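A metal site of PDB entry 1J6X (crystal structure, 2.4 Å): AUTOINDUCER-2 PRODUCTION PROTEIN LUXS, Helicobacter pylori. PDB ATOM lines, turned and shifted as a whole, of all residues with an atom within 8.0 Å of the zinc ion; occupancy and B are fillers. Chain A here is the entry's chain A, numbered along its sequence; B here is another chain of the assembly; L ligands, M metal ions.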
ATOM      1  N   HIS A  55       9.233 -21.213 -16.541  1.00  0.00           N
ATOM      2  CA  HIS A  55      10.185 -20.235 -16.101  1.00  0.00           C
ATOM      3  C   HIS A  55       9.688 -19.521 -14.845  1.00  0.00           C
ATOM      4  O   HIS A  55      10.461 -19.322 -13.894  1.00  0.00           O
ATOM      5  CB  HIS A  55      10.435 -19.201 -17.205  1.00  0.00           C
ATOM      6  CG  HIS A  55      11.558 -18.260 -16.896  1.00  0.00           C
ATOM      7  ND1 HIS A  55      11.848 -17.144 -17.659  1.00  0.00           N
ATOM      8  CD2 HIS A  55      12.488 -18.285 -15.907  1.00  0.00           C
ATOM      9  CE1 HIS A  55      12.882 -16.518 -17.157  1.00  0.00           C
ATOM     10  NE2 HIS A  55      13.303 -17.184 -16.098  1.00  0.00           N
ATOM     11  N   SER A  56       8.422 -19.138 -14.858  1.00  0.00           N
ATOM     12  CA  SER A  56       7.815 -18.446 -13.725  1.00  0.00           C
ATOM     13  C   SER A  56       7.720 -19.358 -12.509  1.00  0.00           C
ATOM     14  O   SER A  56       7.896 -18.897 -11.379  1.00  0.00           O
ATOM     15  CB  SER A  56       6.430 -17.928 -14.088  1.00  0.00           C
ATOM     16  OG  SER A  56       6.551 -16.689 -14.744  1.00  0.00           O
ATOM     17  N   GLU A  58       9.819 -21.766 -11.871  1.00  0.00           N
ATOM     18  CA  GLU A  58      11.192 -21.925 -11.402  1.00  0.00           C
ATOM     19  C   GLU A  58      11.439 -20.812 -10.365  1.00  0.00           C
ATOM     20  O   GLU A  58      11.814 -21.090  -9.227  1.00  0.00           O
ATOM     21  CB  GLU A  58      12.173 -21.745 -12.572  1.00  0.00           C
ATOM     22  CG  GLU A  58      13.633 -21.908 -12.213  1.00  0.00           C
ATOM     23  CD  GLU A  58      14.558 -21.461 -13.344  1.00  0.00           C
ATOM     24  OE1 GLU A  58      15.694 -21.995 -13.448  1.00  0.00           O
ATOM     25  OE2 GLU A  58      14.176 -20.571 -14.126  1.00  0.00           O
ATOM     26  N   HIS A  59      11.210 -19.575 -10.779  1.00  0.00           N
ATOM     27  CA  HIS A  59      11.362 -18.413  -9.902  1.00  0.00           C
ATOM     28  C   HIS A  59      10.563 -18.519  -8.599  1.00  0.00           C
ATOM     29  O   HIS A  59      11.115 -18.418  -7.510  1.00  0.00           O
ATOM     30  CB  HIS A  59      10.887 -17.136 -10.595  1.00  0.00           C
ATOM     31  CG  HIS A  59      11.911 -16.498 -11.464  1.00  0.00           C
ATOM     32  ND1 HIS A  59      12.075 -15.136 -11.523  1.00  0.00           N
ATOM     33  CD2 HIS A  59      12.786 -17.030 -12.348  1.00  0.00           C
ATOM     34  CE1 HIS A  59      13.009 -14.854 -12.413  1.00  0.00           C
ATOM     35  NE2 HIS A  59      13.453 -15.978 -12.919  1.00  0.00           N
ATOM     36  N   VAL A 114       5.610 -12.740 -10.119  1.00  0.00           N
ATOM     37  CA  VAL A 114       6.636 -13.750 -10.251  1.00  0.00           C
ATOM     38  C   VAL A 114       7.819 -12.938  -9.708  1.00  0.00           C
ATOM     39  O   VAL A 114       8.102 -11.845 -10.214  1.00  0.00           O
ATOM     40  CB  VAL A 114       6.903 -14.134 -11.711  1.00  0.00           C
ATOM     41  CG1 VAL A 114       7.981 -15.200 -11.773  1.00  0.00           C
ATOM     42  CG2 VAL A 114       5.627 -14.643 -12.379  1.00  0.00           C
ATOM     43  N   PRO A 115       8.474 -13.421  -8.653  1.00  0.00           N
ATOM     44  CA  PRO A 115       9.596 -12.652  -8.124  1.00  0.00           C
ATOM     45  C   PRO A 115      10.795 -12.618  -9.056  1.00  0.00           C
ATOM     46  O   PRO A 115      11.148 -13.624  -9.665  1.00  0.00           O
ATOM     47  CB  PRO A 115       9.923 -13.343  -6.816  1.00  0.00           C
ATOM     48  CG  PRO A 115       9.562 -14.784  -7.101  1.00  0.00           C
ATOM     49  CD  PRO A 115       8.241 -14.643  -7.856  1.00  0.00           C
ATOM     50  N   ALA A 116      11.429 -11.458  -9.137  1.00  0.00           N
ATOM     51  CA  ALA A 116      12.619 -11.277  -9.942  1.00  0.00           C
ATOM     52  C   ALA A 116      12.391 -11.431 -11.438  1.00  0.00           C
ATOM     53  O   ALA A 116      13.295 -11.851 -12.163  1.00  0.00           O
ATOM     54  CB  ALA A 116      13.712 -12.241  -9.472  1.00  0.00           C
ATOM     55  N   SER A 117      11.196 -11.084 -11.921  1.00  0.00           N
ATOM     56  CA  SER A 117      10.926 -11.169 -13.347  1.00  0.00           C
ATOM     57  C   SER A 117      11.281  -9.861 -14.048  1.00  0.00           C
ATOM     58  O   SER A 117      10.443  -9.278 -14.731  1.00  0.00           O
ATOM     59  CB  SER A 117       9.470 -11.509 -13.584  1.00  0.00           C
ATOM     60  OG  SER A 117       8.635 -10.849 -12.661  1.00  0.00           O
ATOM     61  N   ASN A 118      12.508  -9.384 -13.874  1.00  0.00           N
ATOM     62  CA  ASN A 118      12.957  -8.145 -14.509  1.00  0.00           C
ATOM     63  C   ASN A 118      14.359  -8.343 -15.100  1.00  0.00           C
ATOM     64  O   ASN A 118      15.017  -9.329 -14.796  1.00  0.00           O
ATOM     65  CB  ASN A 118      12.938  -6.995 -13.489  1.00  0.00           C
ATOM     66  CG  ASN A 118      13.818  -7.270 -12.298  1.00  0.00           C
ATOM     67  OD1 ASN A 118      15.048  -7.264 -12.412  1.00  0.00           O
ATOM     68  ND2 ASN A 118      13.212  -7.526 -11.150  1.00  0.00           N
ATOM     69  N   GLN A 121      17.461  -9.070 -12.675  1.00  0.00           N
ATOM     70  CA  GLN A 121      17.611 -10.326 -11.932  1.00  0.00           C
ATOM     71  C   GLN A 121      17.235 -11.600 -12.689  1.00  0.00           C
ATOM     72  O   GLN A 121      17.206 -12.688 -12.109  1.00  0.00           O
ATOM     73  CB  GLN A 121      16.803 -10.255 -10.632  1.00  0.00           C
ATOM     74  CG  GLN A 121      16.697  -8.870 -10.024  1.00  0.00           C
ATOM     75  CD  GLN A 121      15.844  -8.857  -8.778  1.00  0.00           C
ATOM     76  OE1 GLN A 121      16.330  -9.076  -7.662  1.00  0.00           O
ATOM     77  NE2 GLN A 121      14.562  -8.607  -8.954  1.00  0.00           N
ATOM     78  N   CYS A 122      16.969 -11.459 -13.973  1.00  0.00           N
ATOM     79  CA  CYS A 122      16.549 -12.600 -14.777  1.00  0.00           C
ATOM     80  C   CYS A 122      17.149 -12.497 -16.174  1.00  0.00           C
ATOM     81  O   CYS A 122      17.265 -11.407 -16.704  1.00  0.00           O
ATOM     82  CB  CYS A 122      15.024 -12.610 -14.841  1.00  0.00           C
ATOM     83  SG  CYS A 122      14.295 -13.812 -15.914  1.00  0.00           S
ATOM     84  N   GLY A 123      17.540 -13.629 -16.739  1.00  0.00           N
ATOM     85  CA  GLY A 123      18.135 -13.654 -18.063  1.00  0.00           C
ATOM     86  C   GLY A 123      17.174 -13.515 -19.235  1.00  0.00           C
ATOM     87  O   GLY A 123      17.623 -13.290 -20.374  1.00  0.00           O
ATOM     88  N   TRP A 124      15.872 -13.686 -19.003  1.00  0.00           N
ATOM     89  CA  TRP A 124      14.845 -13.515 -20.045  1.00  0.00           C
ATOM     90  C   TRP A 124      13.582 -13.018 -19.339  1.00  0.00           C
ATOM     91  O   TRP A 124      12.573 -13.726 -19.253  1.00  0.00           O
ATOM     92  CB  TRP A 124      14.562 -14.823 -20.789  1.00  0.00           C
ATOM     93  CG  TRP A 124      13.795 -14.587 -22.068  1.00  0.00           C
ATOM     94  CD1 TRP A 124      13.335 -13.383 -22.538  1.00  0.00           C
ATOM     95  CD2 TRP A 124      13.352 -15.571 -23.020  1.00  0.00           C
ATOM     96  NE1 TRP A 124      12.630 -13.557 -23.709  1.00  0.00           N
ATOM     97  CE2 TRP A 124      12.631 -14.884 -24.035  1.00  0.00           C
ATOM     98  CE3 TRP A 124      13.494 -16.967 -23.120  1.00  0.00           C
ATOM     99  CZ2 TRP A 124      12.049 -15.551 -25.125  1.00  0.00           C
ATOM    100  CZ3 TRP A 124      12.918 -17.627 -24.206  1.00  0.00           C
ATOM    101  CH2 TRP A 124      12.206 -16.919 -25.199  1.00  0.00           C
ATOM    102  N   ALA A 125      13.659 -11.776 -18.842  1.00  0.00           N
ATOM    103  CA  ALA A 125      12.585 -11.162 -18.074  1.00  0.00           C
ATOM    104  C   ALA A 125      11.201 -11.143 -18.702  1.00  0.00           C
ATOM    105  O   ALA A 125      10.201 -11.284 -17.997  1.00  0.00           O
ATOM    106  CB  ALA A 125      12.997  -9.742 -17.665  1.00  0.00           C
ATOM    107  N   ALA A 126      11.141 -10.963 -20.018  1.00  0.00           N
ATOM    108  CA  ALA A 126       9.861 -10.927 -20.701  1.00  0.00           C
ATOM    109  C   ALA A 126       9.145 -12.279 -20.750  1.00  0.00           C
ATOM    110  O   ALA A 126       7.918 -12.325 -20.833  1.00  0.00           O
ATOM    111  CB  ALA A 126      10.049 -10.401 -22.137  1.00  0.00           C
ATOM    112  N   ASN A 127       9.891 -13.374 -20.676  1.00  0.00           N
ATOM    113  CA  ASN A 127       9.301 -14.715 -20.774  1.00  0.00           C
ATOM    114  C   ASN A 127       8.760 -15.255 -19.459  1.00  0.00           C
ATOM    115  O   ASN A 127       9.330 -16.168 -18.871  1.00  0.00           O
ATOM    116  CB  ASN A 127      10.324 -15.678 -21.357  1.00  0.00           C
ATOM    117  CG  ASN A 127       9.688 -16.745 -22.227  1.00  0.00           C
ATOM    118  OD1 ASN A 127       8.829 -16.430 -23.054  1.00  0.00           O
ATOM    119  ND2 ASN A 127      10.104 -17.997 -22.061  1.00  0.00           N
ATOM    120  N   HIS A 128       7.643 -14.710 -19.008  1.00  0.00           N
ATOM    121  CA  HIS A 128       7.024 -15.138 -17.757  1.00  0.00           C
ATOM    122  C   HIS A 128       5.489 -15.057 -17.799  1.00  0.00           C
ATOM    123  O   HIS A 128       4.907 -14.432 -18.682  1.00  0.00           O
ATOM    124  CB  HIS A 128       7.473 -14.226 -16.615  1.00  0.00           C
ATOM    125  CG  HIS A 128       8.817 -14.556 -16.044  1.00  0.00           C
ATOM    126  ND1 HIS A 128       9.027 -15.655 -15.244  1.00  0.00           N
ATOM    127  CD2 HIS A 128      10.004 -13.922 -16.151  1.00  0.00           C
ATOM    128  CE1 HIS A 128      10.304 -15.688 -14.882  1.00  0.00           C
ATOM    129  NE2 HIS A 128      10.916 -14.645 -15.421  1.00  0.00           N
ATOM    130  N   SER B   7      21.167 -16.166  -7.641  1.00  0.00           N
ATOM    131  CA  SER B   7      21.168 -15.469  -8.917  1.00  0.00           C
ATOM    132  C   SER B   7      20.306 -14.206  -8.967  1.00  0.00           C
ATOM    133  O   SER B   7      20.514 -13.359  -9.848  1.00  0.00           O
ATOM    134  CB  SER B   7      20.787 -16.414 -10.040  1.00  0.00           C
ATOM    135  OG  SER B   7      19.383 -16.550 -10.134  1.00  0.00           O
ATOM    136  N   PHE B   8      19.344 -14.058  -8.063  1.00  0.00           N
ATOM    137  CA  PHE B   8      18.513 -12.867  -8.061  1.00  0.00           C
ATOM    138  C   PHE B   8      19.306 -11.680  -7.527  1.00  0.00           C
ATOM    139  O   PHE B   8      18.842 -10.544  -7.527  1.00  0.00           O
ATOM    140  CB  PHE B   8      17.249 -13.071  -7.203  1.00  0.00           C
ATOM    141  CG  PHE B   8      16.279 -14.077  -7.752  1.00  0.00           C
ATOM    142  CD1 PHE B   8      16.494 -14.698  -8.985  1.00  0.00           C
ATOM    143  CD2 PHE B   8      15.114 -14.391  -7.049  1.00  0.00           C
ATOM    144  CE1 PHE B   8      15.571 -15.604  -9.504  1.00  0.00           C
ATOM    145  CE2 PHE B   8      14.184 -15.297  -7.560  1.00  0.00           C
ATOM    146  CZ  PHE B   8      14.421 -15.896  -8.787  1.00  0.00           C
ATOM    147  N   HIS B  12      22.132  -8.840 -13.852  1.00  0.00           N
ATOM    148  CA  HIS B  12      22.205  -9.371 -15.192  1.00  0.00           C
ATOM    149  C   HIS B  12      22.584  -8.398 -16.305  1.00  0.00           C
ATOM    150  O   HIS B  12      23.090  -8.823 -17.348  1.00  0.00           O
ATOM    151  CB  HIS B  12      20.900 -10.096 -15.521  1.00  0.00           C
ATOM    152  CG  HIS B  12      20.735 -11.407 -14.813  1.00  0.00           C
ATOM    153  ND1 HIS B  12      20.846 -11.523 -13.438  1.00  0.00           N
ATOM    154  CD2 HIS B  12      20.476 -12.646 -15.283  1.00  0.00           C
ATOM    155  CE1 HIS B  12      20.653 -12.782 -13.097  1.00  0.00           C
ATOM    156  NE2 HIS B  12      20.433 -13.484 -14.193  1.00  0.00           N
ATOM    157  N   ARG B  40      27.102 -19.317 -18.331  1.00  0.00           N
ATOM    158  CA  ARG B  40      26.266 -18.513 -19.204  1.00  0.00           C
ATOM    159  C   ARG B  40      26.651 -18.563 -20.685  1.00  0.00           C
ATOM    160  O   ARG B  40      27.758 -18.147 -21.052  1.00  0.00           O
ATOM    161  CB  ARG B  40      26.361 -17.066 -18.699  1.00  0.00           C
ATOM    162  CG  ARG B  40      25.353 -16.085 -19.266  1.00  0.00           C
ATOM    163  CD  ARG B  40      23.971 -16.290 -18.682  1.00  0.00           C
ATOM    164  NE  ARG B  40      23.997 -16.359 -17.220  1.00  0.00           N
ATOM    165  CZ  ARG B  40      22.915 -16.233 -16.447  1.00  0.00           C
ATOM    166  NH1 ARG B  40      21.728 -16.020 -16.991  1.00  0.00           N
ATOM    167  NH2 ARG B  40      23.026 -16.349 -15.136  1.00  0.00           N
ATOM    168  N   ASN B  45      18.709 -11.311 -21.562  1.00  0.00           N
ATOM    169  CA  ASN B  45      17.722 -10.449 -22.207  1.00  0.00           C
ATOM    170  C   ASN B  45      18.151  -9.904 -23.554  1.00  0.00           C
ATOM    171  O   ASN B  45      17.583  -8.936 -24.058  1.00  0.00           O
ATOM    172  CB  ASN B  45      17.393  -9.276 -21.283  1.00  0.00           C
ATOM    173  CG  ASN B  45      16.798  -9.746 -19.972  1.00  0.00           C
ATOM    174  OD1 ASN B  45      15.704 -10.286 -19.942  1.00  0.00           O
ATOM    175  ND2 ASN B  45      17.535  -9.535 -18.892  1.00  0.00           N
ATOM    176  N   MET B  78      19.009 -23.418 -17.192  1.00  0.00           N
ATOM    177  CA  MET B  78      18.293 -22.357 -16.500  1.00  0.00           C
ATOM    178  C   MET B  78      16.960 -22.181 -17.211  1.00  0.00           C
ATOM    179  O   MET B  78      16.858 -22.384 -18.429  1.00  0.00           O
ATOM    180  CB  MET B  78      19.086 -21.067 -16.572  1.00  0.00           C
ATOM    181  CG  MET B  78      20.369 -21.096 -15.753  1.00  0.00           C
ATOM    182  SD  MET B  78      21.427 -19.529 -16.092  1.00  0.00           S
ATOM    183  CE  MET B  78      23.005 -20.028 -15.098  1.00  0.00           C
ATOM    184  N   GLY B  79      15.934 -21.792 -16.474  1.00  0.00           N
ATOM    185  CA  GLY B  79      14.645 -21.595 -17.095  1.00  0.00           C
ATOM    186  C   GLY B  79      14.681 -20.425 -18.063  1.00  0.00           C
ATOM    187  O   GLY B  79      13.872 -20.342 -18.998  1.00  0.00           O
ATOM    188  N   CYS B  80      15.618 -19.516 -17.862  1.00  0.00           N
ATOM    189  CA  CYS B  80      15.738 -18.346 -18.732  1.00  0.00           C
ATOM    190  C   CYS B  80      16.392 -18.687 -20.066  1.00  0.00           C
ATOM    191  O   CYS B  80      16.596 -17.820 -20.910  1.00  0.00           O
ATOM    192  CB  CYS B  80      16.527 -17.246 -18.019  1.00  0.00           C
ATOM    193  SG  CYS B  80      18.167 -17.740 -17.421  1.00  0.00           S
ATOM    194  N   GLN B  81      16.743 -19.958 -20.247  1.00  0.00           N
ATOM    195  CA  GLN B  81      17.351 -20.422 -21.493  1.00  0.00           C
ATOM    196  C   GLN B  81      18.663 -19.733 -21.886  1.00  0.00           C
ATOM    197  O   GLN B  81      19.070 -19.806 -23.057  1.00  0.00           O
ATOM    198  CB  GLN B  81      16.353 -20.299 -22.644  1.00  0.00           C
ATOM    199  CG  GLN B  81      15.024 -20.973 -22.384  1.00  0.00           C
ATOM    200  CD  GLN B  81      14.054 -20.947 -23.565  1.00  0.00           C
ATOM    201  OE1 GLN B  81      12.855 -20.770 -23.381  1.00  0.00           O
ATOM    202  NE2 GLN B  81      14.571 -21.152 -24.764  1.00  0.00           N
ATOM    203  N   THR B  82      19.341 -19.062 -20.951  1.00  0.00           N
ATOM    204  CA  THR B  82      20.579 -18.417 -21.343  1.00  0.00           C
ATOM    205  C   THR B  82      21.794 -19.125 -20.802  1.00  0.00           C
ATOM    206  O   THR B  82      22.919 -18.758 -21.114  1.00  0.00           O
ATOM    207  CB  THR B  82      20.666 -16.934 -20.883  1.00  0.00           C
ATOM    208  OG1 THR B  82      20.612 -16.863 -19.460  1.00  0.00           O
ATOM    209  CG2 THR B  82      19.520 -16.118 -21.495  1.00  0.00           C
HETATM  210  N1  LIG L   1      18.304 -23.573  -9.567  1.00  0.00           N
HETATM  211  C1  LIG L   1      18.334 -22.162  -9.105  1.00  0.00           C
HETATM  212  C2  LIG L   1      18.292 -22.092  -7.566  1.00  0.00           C
HETATM  213  O1  LIG L   1      17.710 -23.001  -6.944  1.00  0.00           O
HETATM  214  C3  LIG L   1      17.125 -21.432  -9.708  1.00  0.00           C
HETATM  215  C4  LIG L   1      16.975 -19.996  -9.296  1.00  0.00           C
HETATM  216  S1  LIG L   1      15.502 -19.215 -10.006  1.00  0.00           S
HETATM  217  C5  LIG L   1      16.161 -18.565 -11.534  1.00  0.00           C
HETATM  218  O2  LIG L   1      18.843 -21.130  -6.997  1.00  0.00           O
HETATM  219 ZN    ZN M   1      14.517 -16.009 -14.883  1.00  0.00          ZN
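Residues that only touch the zinc ion: His 128 and Cys 80 of chain B.
Five residues have an atom within 4 Å of the zinc ion: His 55, His 59, Cys 122, His 128 and Cys 80 of chain B.
Along chain A the residues within 4 Å of the zinc ion span positions 55 to 128.
The nearest printed residue that does not touch the zinc ion is Gly 123 (4.3 Å).
ND1 of His 55 lies close to NE2 of His 128 (3.5 Å).
ND1 of His 55 is in hydrogen-bond range of O of Asn 127 (3.0 Å).
A ring nitrogen (ND1) of His 59 lies within hydrogen-bond range of the backbone carbonyl oxygen of Pro 115 (2.6 Å).
A ring nitrogen (NE2) of His 128 sits close to the side-chain sulfur (SG) of Cys 122, at 3.5 Å.
N of Trp 124 lies close to SG of Cys 122, 3.5 Å away.
The backbone NH (N) of Ala 125 sits close to the side-chain sulfur (SG) of Cys 122 (3.6 Å).
A ring nitrogen (ND1) of His 128 is in hydrogen-bond range of the side-chain hydroxyl of Ser 56 (2.7 Å).
OG1 of Thr 82 of chain B is in hydrogen-bond range of SG of Cys 80 of chain B, 3.3 Å away.
The zinc ion is bound by a ring nitrogen (NE2) of His 55 (2.1 Å), a ring nitrogen (NE2) of His 59 (2.2 Å) and the side-chain sulfur of Cys 122 (2.4 Å).
The zinc ion has three donor atoms within binding distance.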
